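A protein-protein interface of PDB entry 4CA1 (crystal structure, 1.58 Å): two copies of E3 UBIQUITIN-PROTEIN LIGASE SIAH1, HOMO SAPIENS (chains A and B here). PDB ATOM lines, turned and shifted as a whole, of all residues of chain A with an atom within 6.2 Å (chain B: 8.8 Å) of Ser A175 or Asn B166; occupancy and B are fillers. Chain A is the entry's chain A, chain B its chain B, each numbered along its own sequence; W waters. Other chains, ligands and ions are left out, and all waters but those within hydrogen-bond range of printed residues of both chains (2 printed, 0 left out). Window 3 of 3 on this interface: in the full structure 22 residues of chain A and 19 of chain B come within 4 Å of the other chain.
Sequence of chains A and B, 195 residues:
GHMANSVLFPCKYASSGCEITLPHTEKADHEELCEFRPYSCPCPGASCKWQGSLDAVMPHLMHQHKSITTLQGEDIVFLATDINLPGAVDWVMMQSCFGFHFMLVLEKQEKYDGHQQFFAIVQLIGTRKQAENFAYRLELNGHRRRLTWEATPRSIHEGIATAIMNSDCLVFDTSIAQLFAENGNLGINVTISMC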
ATOM      1  N   GLN A 116      -9.767  16.839   0.086  1.00  0.00           N
ATOM      2  CA  GLN A 116     -10.399  15.915   0.959  1.00  0.00           C
ATOM      3  C   GLN A 116      -9.662  15.986   2.310  1.00  0.00           C
ATOM      4  O   GLN A 116      -8.425  16.204   2.330  1.00  0.00           O
ATOM      5  CB  GLN A 116     -10.299  14.493   0.346  1.00  0.00           C
ATOM      6  CG  GLN A 116     -10.661  14.346  -1.150  1.00  0.00           C
ATOM      7  CD  GLN A 116     -12.147  14.350  -1.393  1.00  0.00           C
ATOM      8  OE1 GLN A 116     -12.928  13.777  -0.617  1.00  0.00           O
ATOM      9  NE2 GLN A 116     -12.559  14.990  -2.493  1.00  0.00           N
ATOM     10  N   ASP A 173      -4.860  15.603   5.791  1.00  0.00           N
ATOM     11  CA  ASP A 173      -5.345  15.878   4.435  1.00  0.00           C
ATOM     12  C   ASP A 173      -4.885  14.792   3.440  1.00  0.00           C
ATOM     13  O   ASP A 173      -4.126  13.884   3.777  1.00  0.00           O
ATOM     14  CB  ASP A 173      -4.847  17.328   4.028  1.00  0.00           C
ATOM     15  CG  ASP A 173      -3.338  17.567   4.160  1.00  0.00           C
ATOM     16  OD1 ASP A 173      -2.614  16.616   3.869  1.00  0.00           O
ATOM     17  OD2 ASP A 173      -2.827  18.774   4.413  1.00  0.00           O
ATOM     18  N   THR A 174      -5.313  14.935   2.193  1.00  0.00           N
ATOM     19  CA  THR A 174      -4.863  14.054   1.116  1.00  0.00           C
ATOM     20  C   THR A 174      -3.354  14.032   0.944  1.00  0.00           C
ATOM     21  O   THR A 174      -2.794  12.969   0.667  1.00  0.00           O
ATOM     22  CB  THR A 174      -5.500  14.443  -0.281  1.00  0.00           C
ATOM     23  OG1 THR A 174      -6.900  14.277  -0.208  1.00  0.00           O
ATOM     24  CG2 THR A 174      -5.032  13.542  -1.449  1.00  0.00           C
ATOM     25  N   SER A 175      -2.672  15.180   1.113  1.00  0.00           N
ATOM     26  CA  SER A 175      -1.210  15.179   0.941  1.00  0.00           C
ATOM     27  C   SER A 175      -0.561  14.309   1.999  1.00  0.00           C
ATOM     28  O   SER A 175       0.388  13.553   1.715  1.00  0.00           O
ATOM     29  CB  SER A 175      -0.624  16.579   1.061  1.00  0.00           C
ATOM     30  OG  SER A 175      -0.793  17.214  -0.169  1.00  0.00           O
ATOM     31  N   ILE A 176      -1.059  14.424   3.225  1.00  0.00           N
ATOM     32  CA  ILE A 176      -0.556  13.565   4.305  1.00  0.00           C
ATOM     33  C   ILE A 176      -0.802  12.092   4.034  1.00  0.00           C
ATOM     34  O   ILE A 176       0.135  11.263   4.156  1.00  0.00           O
ATOM     35  CB  ILE A 176      -1.140  14.033   5.671  1.00  0.00           C
ATOM     36  CG1 ILE A 176      -0.484  15.346   6.027  1.00  0.00           C
ATOM     37  CG2 ILE A 176      -0.776  13.017   6.768  1.00  0.00           C
ATOM     38  CD1 ILE A 176      -1.217  16.175   7.088  1.00  0.00           C
ATOM     39  N   ALA A 177      -2.023  11.758   3.621  1.00  0.00           N
ATOM     40  CA  ALA A 177      -2.401  10.373   3.356  1.00  0.00           C
ATOM     41  C   ALA A 177      -1.452   9.826   2.314  1.00  0.00           C
ATOM     42  O   ALA A 177      -0.998   8.689   2.474  1.00  0.00           O
ATOM     43  CB  ALA A 177      -3.802  10.288   2.864  1.00  0.00           C
ATOM     44  N   GLN A 178      -1.132  10.611   1.286  1.00  0.00           N
ATOM     45  CA  GLN A 178      -0.190  10.144   0.242  1.00  0.00           C
ATOM     46  C   GLN A 178       1.233   9.890   0.755  1.00  0.00           C
ATOM     47  O   GLN A 178       1.850   8.948   0.280  1.00  0.00           O
ATOM     48  CB  GLN A 178      -0.045  11.160  -0.896  1.00  0.00           C
ATOM     49  CG  GLN A 178      -1.252  11.353  -1.778  1.00  0.00           C
ATOM     50  CD  GLN A 178      -2.191  10.185  -1.713  1.00  0.00           C
ATOM     51  OE1 GLN A 178      -1.923   9.095  -2.278  1.00  0.00           O
ATOM     52  NE2 GLN A 178      -3.300  10.381  -0.989  1.00  0.00           N
ATOM     53  N   LEU A 179       1.734  10.728   1.689  1.00  0.00           N
ATOM     54  CA  LEU A 179       3.067  10.510   2.297  1.00  0.00           C
ATOM     55  C   LEU A 179       3.174   9.171   2.964  1.00  0.00           C
ATOM     56  O   LEU A 179       4.235   8.592   2.974  1.00  0.00           O
ATOM     57  CB  LEU A 179       3.477  11.559   3.365  1.00  0.00           C
ATOM     58  CG  LEU A 179       3.782  12.924   2.944  1.00  0.00           C
ATOM     59  CD1 LEU A 179       3.766  13.797   4.243  1.00  0.00           C
ATOM     60  CD2 LEU A 179       5.112  12.874   2.202  1.00  0.00           C
ATOM     61  N   PHE A 180       2.054   8.699   3.529  1.00  0.00           N
ATOM     62  CA  PHE A 180       2.062   7.516   4.355  1.00  0.00           C
ATOM     63  C   PHE A 180       1.535   6.301   3.602  1.00  0.00           C
ATOM     64  O   PHE A 180       1.736   5.214   4.056  1.00  0.00           O
ATOM     65  CB  PHE A 180       1.259   7.733   5.615  1.00  0.00           C
ATOM     66  CG  PHE A 180       2.019   8.661   6.580  1.00  0.00           C
ATOM     67  CD1 PHE A 180       3.098   8.154   7.247  1.00  0.00           C
ATOM     68  CD2 PHE A 180       1.615   9.977   6.824  1.00  0.00           C
ATOM     69  CE1 PHE A 180       3.811   8.943   8.159  1.00  0.00           C
ATOM     70  CE2 PHE A 180       2.381  10.820   7.698  1.00  0.00           C
ATOM     71  CZ  PHE A 180       3.433  10.288   8.408  1.00  0.00           C
ATOM     72  N   GLN B 109      -1.381  29.853   8.625  1.00  0.00           N
ATOM     73  CA  GLN B 109      -1.711  30.330   7.318  1.00  0.00           C
ATOM     74  C   GLN B 109      -3.173  30.662   7.225  1.00  0.00           C
ATOM     75  O   GLN B 109      -3.969  30.217   8.035  1.00  0.00           O
ATOM     76  CB  GLN B 109      -1.436  29.287   6.288  1.00  0.00           C
ATOM     77  CG  GLN B 109       0.033  29.046   6.055  1.00  0.00           C
ATOM     78  CD  GLN B 109       0.232  28.129   4.860  1.00  0.00           C
ATOM     79  OE1 GLN B 109      -0.755  27.564   4.315  1.00  0.00           O
ATOM     80  NE2 GLN B 109       1.510  27.969   4.432  1.00  0.00           N
ATOM     81  N   PHE B 119       1.308  25.036  10.699  1.00  0.00           N
ATOM     82  CA  PHE B 119       2.322  24.107  10.190  1.00  0.00           C
ATOM     83  C   PHE B 119       3.517  24.289  11.072  1.00  0.00           C
ATOM     84  O   PHE B 119       4.013  25.395  11.236  1.00  0.00           O
ATOM     85  CB  PHE B 119       2.712  24.487   8.751  1.00  0.00           C
ATOM     86  CG  PHE B 119       1.554  24.405   7.810  1.00  0.00           C
ATOM     87  CD1 PHE B 119       0.585  25.487   7.712  1.00  0.00           C
ATOM     88  CD2 PHE B 119       1.389  23.270   6.983  1.00  0.00           C
ATOM     89  CE1 PHE B 119      -0.515  25.340   6.877  1.00  0.00           C
ATOM     90  CE2 PHE B 119       0.271  23.139   6.118  1.00  0.00           C
ATOM     91  CZ  PHE B 119      -0.695  24.184   6.067  1.00  0.00           C
ATOM     92  N   ILE B 121       7.556  22.872  11.794  1.00  0.00           N
ATOM     93  CA  ILE B 121       8.604  22.138  11.125  1.00  0.00           C
ATOM     94  C   ILE B 121       9.930  22.573  11.695  1.00  0.00           C
ATOM     95  O   ILE B 121      10.046  23.653  12.309  1.00  0.00           O
ATOM     96  CB  ILE B 121       8.546  22.411   9.586  1.00  0.00           C
ATOM     97  CG1 ILE B 121       9.407  21.345   8.802  1.00  0.00           C
ATOM     98  CG2 ILE B 121       8.768  23.942   9.296  1.00  0.00           C
ATOM     99  CD1 ILE B 121       9.153  21.463   7.262  1.00  0.00           C
ATOM    100  N   TRP B 149       4.552  14.583  15.858  1.00  0.00           N
ATOM    101  CA  TRP B 149       5.117  14.430  14.543  1.00  0.00           C
ATOM    102  C   TRP B 149       6.604  14.168  14.733  1.00  0.00           C
ATOM    103  O   TRP B 149       7.285  14.894  15.511  1.00  0.00           O
ATOM    104  CB  TRP B 149       4.922  15.787  13.786  1.00  0.00           C
ATOM    105  CG  TRP B 149       5.717  15.848  12.530  1.00  0.00           C
ATOM    106  CD1 TRP B 149       6.816  16.624  12.306  1.00  0.00           C
ATOM    107  CD2 TRP B 149       5.439  15.198  11.273  1.00  0.00           C
ATOM    108  NE1 TRP B 149       7.267  16.507  10.991  1.00  0.00           N
ATOM    109  CE2 TRP B 149       6.466  15.603  10.351  1.00  0.00           C
ATOM    110  CE3 TRP B 149       4.446  14.312  10.848  1.00  0.00           C
ATOM    111  CZ2 TRP B 149       6.503  15.173   9.012  1.00  0.00           C
ATOM    112  CZ3 TRP B 149       4.510  13.840   9.477  1.00  0.00           C
ATOM    113  CH2 TRP B 149       5.500  14.303   8.596  1.00  0.00           C
ATOM    114  N   ARG B 154      14.573  19.444   7.812  1.00  0.00           N
ATOM    115  CA  ARG B 154      14.986  19.894   6.470  1.00  0.00           C
ATOM    116  C   ARG B 154      16.277  20.705   6.578  1.00  0.00           C
ATOM    117  O   ARG B 154      16.496  21.419   7.554  1.00  0.00           O
ATOM    118  CB  ARG B 154      13.889  20.808   5.854  1.00  0.00           C
ATOM    119  CG  ARG B 154      12.617  20.066   5.542  1.00  0.00           C
ATOM    120  CD  ARG B 154      12.787  19.431   4.172  1.00  0.00           C
ATOM    121  NE  ARG B 154      11.704  18.489   3.989  1.00  0.00           N
ATOM    122  CZ  ARG B 154      11.416  17.941   2.836  1.00  0.00           C
ATOM    123  NH1 ARG B 154      12.161  18.272   1.799  1.00  0.00           N
ATOM    124  NH2 ARG B 154      10.388  17.085   2.723  1.00  0.00           N
ATOM    125  N   ILE B 160      11.848  25.215   3.848  1.00  0.00           N
ATOM    126  CA  ILE B 160      10.664  24.616   4.451  1.00  0.00           C
ATOM    127  C   ILE B 160       9.386  24.925   3.638  1.00  0.00           C
ATOM    128  O   ILE B 160       8.323  24.363   3.877  1.00  0.00           O
ATOM    129  CB  ILE B 160      10.484  25.043   5.960  1.00  0.00           C
ATOM    130  CG1 ILE B 160      10.246  26.578   6.040  1.00  0.00           C
ATOM    131  CG2 ILE B 160      11.685  24.541   6.856  1.00  0.00           C
ATOM    132  CD1 ILE B 160       9.998  27.014   7.463  1.00  0.00           C
ATOM    133  N   ALA B 161       9.471  25.805   2.651  1.00  0.00           N
ATOM    134  CA  ALA B 161       8.274  26.177   1.898  1.00  0.00           C
ATOM    135  C   ALA B 161       7.685  24.998   1.157  1.00  0.00           C
ATOM    136  O   ALA B 161       6.446  24.832   1.108  1.00  0.00           O
ATOM    137  CB  ALA B 161       8.597  27.282   0.909  1.00  0.00           C
ATOM    138  N   THR B 162       8.572  24.191   0.562  1.00  0.00           N
ATOM    139  CA  THR B 162       8.041  23.015  -0.244  1.00  0.00           C
ATOM    140  C   THR B 162       7.438  22.037   0.727  1.00  0.00           C
ATOM    141  O   THR B 162       6.357  21.512   0.482  1.00  0.00           O
ATOM    142  CB  THR B 162       9.160  22.356  -1.017  1.00  0.00           C
ATOM    143  OG1 THR B 162       9.616  23.345  -1.929  1.00  0.00           O
ATOM    144  CG2 THR B 162       8.680  21.133  -1.802  1.00  0.00           C
ATOM    145  N   ALA B 163       8.114  21.762   1.846  1.00  0.00           N
ATOM    146  CA  ALA B 163       7.554  20.830   2.818  1.00  0.00           C
ATOM    147  C   ALA B 163       6.195  21.270   3.317  1.00  0.00           C
ATOM    148  O   ALA B 163       5.233  20.485   3.387  1.00  0.00           O
ATOM    149  CB  ALA B 163       8.545  20.615   3.953  1.00  0.00           C
ATOM    150  N   ILE B 164       6.077  22.568   3.640  1.00  0.00           N
ATOM    151  CA  ILE B 164       4.773  23.112   4.105  1.00  0.00           C
ATOM    152  C   ILE B 164       3.679  22.998   3.012  1.00  0.00           C
ATOM    153  O   ILE B 164       2.572  22.540   3.295  1.00  0.00           O
ATOM    154  CB  ILE B 164       5.003  24.560   4.578  1.00  0.00           C
ATOM    155  CG1 ILE B 164       5.741  24.513   5.930  1.00  0.00           C
ATOM    156  CG2 ILE B 164       3.641  25.269   4.694  1.00  0.00           C
ATOM    157  CD1 ILE B 164       6.278  25.814   6.526  1.00  0.00           C
ATOM    158  N   MET B 165       4.048  23.265   1.752  1.00  0.00           N
ATOM    159  CA  MET B 165       3.141  23.151   0.641  1.00  0.00           C
ATOM    160  C   MET B 165       2.622  21.713   0.527  1.00  0.00           C
ATOM    161  O   MET B 165       1.461  21.472   0.153  1.00  0.00           O
ATOM    162  CB  MET B 165       3.834  23.589  -0.664  1.00  0.00           C
ATOM    163  CG  MET B 165       2.969  23.481  -1.886  1.00  0.00           C
ATOM    164  SD  MET B 165       3.970  23.968  -3.309  1.00  0.00           S
ATOM    165  CE  MET B 165       4.818  25.477  -2.759  1.00  0.00           C
ATOM    166  N   ASN B 166       3.493  20.756   0.867  1.00  0.00           N
ATOM    167  CA  ASN B 166       3.174  19.339   0.754  1.00  0.00           C
ATOM    168  C   ASN B 166       2.668  18.695   2.047  1.00  0.00           C
ATOM    169  O   ASN B 166       2.432  17.473   2.100  1.00  0.00           O
ATOM    170  CB  ASN B 166       4.429  18.605   0.259  1.00  0.00           C
ATOM    171  CG  ASN B 166       4.706  18.894  -1.208  1.00  0.00           C
ATOM    172  OD1 ASN B 166       3.781  19.121  -1.993  1.00  0.00           O
ATOM    173  ND2 ASN B 166       5.969  18.880  -1.595  1.00  0.00           N
ATOM    174  N   SER B 167       2.435  19.516   3.093  1.00  0.00           N
ATOM    175  CA  SER B 167       2.008  19.015   4.429  1.00  0.00           C
ATOM    176  C   SER B 167       2.962  17.973   4.980  1.00  0.00           C
ATOM    177  O   SER B 167       2.547  17.173   5.823  1.00  0.00           O
ATOM    178  CB  SER B 167       0.595  18.459   4.419  1.00  0.00           C
ATOM    179  OG  SER B 167      -0.290  19.524   4.026  1.00  0.00           O
ATOM    180  N   ASP B 168       4.252  18.116   4.615  1.00  0.00           N
ATOM    181  CA  ASP B 168       5.300  17.224   5.119  1.00  0.00           C
ATOM    182  C   ASP B 168       5.918  17.803   6.409  1.00  0.00           C
ATOM    183  O   ASP B 168       7.082  18.171   6.464  1.00  0.00           O
ATOM    184  CB  ASP B 168       6.293  16.973   4.009  1.00  0.00           C
ATOM    185  CG  ASP B 168       7.238  15.809   4.286  1.00  0.00           C
ATOM    186  OD1 ASP B 168       7.140  15.143   5.335  1.00  0.00           O
ATOM    187  OD2 ASP B 168       8.060  15.590   3.382  1.00  0.00           O
ATOM    188  N   CYS B 169       5.089  17.860   7.430  1.00  0.00           N
ATOM    189  CA  CYS B 169       5.386  18.525   8.691  1.00  0.00           C
ATOM    190  C   CYS B 169       4.199  18.278   9.594  1.00  0.00           C
ATOM    191  O   CYS B 169       3.250  17.563   9.211  1.00  0.00           O
ATOM    192  CB  CYS B 169       5.681  20.048   8.488  1.00  0.00           C
ATOM    193  SG  CYS B 169       4.248  20.960   7.825  1.00  0.00           S
ATOM    194  N   VAL B 171       0.797  19.319  10.948  1.00  0.00           N
ATOM    195  CA  VAL B 171      -0.239  20.214  10.415  1.00  0.00           C
ATOM    196  C   VAL B 171      -1.458  20.075  11.330  1.00  0.00           C
ATOM    197  O   VAL B 171      -1.953  18.934  11.570  1.00  0.00           O
ATOM    198  CB  VAL B 171      -0.651  19.832   8.972  1.00  0.00           C
ATOM    199  CG1 VAL B 171      -1.719  20.821   8.448  1.00  0.00           C
ATOM    200  CG2 VAL B 171       0.529  19.760   8.000  1.00  0.00           C
HETATM  201  O   HOH W   1       1.197  17.062  -1.901  1.00  0.00           O
HETATM  202  O   HOH W   2      -0.525  19.770   1.263  1.00  0.00           O
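OD2 of Asp A173 is in hydrogen-bond range of OG of Ser B167 (2.7 Å).
Water W1 lies within hydrogen-bond range of OG of Ser A175 and OD1 of Asn B166. Water W2 lies within hydrogen-bond range of the side-chain hydroxyl (OG) of Ser B167 (2.8 Å), the backbone carbonyl oxygen (O) of Met B165 (2.8 Å) and the side-chain hydroxyl (OG) of Ser A175 (2.9 Å).
Along chain B the printed residues that touch a printed residue of chain A span positions 149 to 168. Of the 9 printed residues of chain A, 5 touch a printed residue of chain B. Hydrophobic or aromatic side chains of chain A within 4 Å of the printed part of chain B: Ile A176, Leu A179 and Phe A180. Among the printed residues, 6 pairs touch across the chains.
O of Ala B163 lies within hydrogen-bond range of N of Asp B168, 2.8 Å away. The backbone carbonyl oxygen of Thr B162 sits at hydrogen-bond distance from the side-chain amide nitrogen of Asn B166, 3.4 Å away. OD1 of Asp A173 is in hydrogen-bond range of N of Ile A176 (2.8 Å). OD1 of Asp A173 lies within hydrogen-bond range of N of Ser A175, at 3.1 Å. The guanidinium group of Arg B154 is in salt-bridge range of the side-chain carboxylate of Asp B168.
No position is printed for both chains. Of the 6 pairs that touch across the chains among the printed residues, none has its exchanged pair printed and touching as well.
Among the printed residues, pairs that only touch across the chains: Ser A175 with Asn B166 (3.3 Å), Ile A176 with Ser B167 (3.5 Å), Leu A179 with Asp B168 (3.8 Å), Phe A180 with Trp B149 (3.9 Å) and Leu A179 with Ser B167 (3.9 Å).
Thr A174 touches none of the printed residues of chain B. Of the printed residues of chain B, Ser A175 touches Asn B166 (3.3 Å). Of the printed residues of chain B, Leu A179 touches Ser B167 (3.9 Å) and Asp B168 (3.8 Å). Of the printed residues of chain B, Phe A180 touches Trp B149 (3.9 Å). Ile B121 touches none of the printed residues of chain A. Of the printed residues of chain A, Trp B149 touches Phe A180 (3.9 Å). Printed residues of chain A within 4 Å of Asn B166: Ser A175. Of the printed residues of chain A, Asp B168 touches Leu A179 (3.8 Å). The nearest printed residue of chain B that does not touch Ile A176 is Val B171 (4.1 Å).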
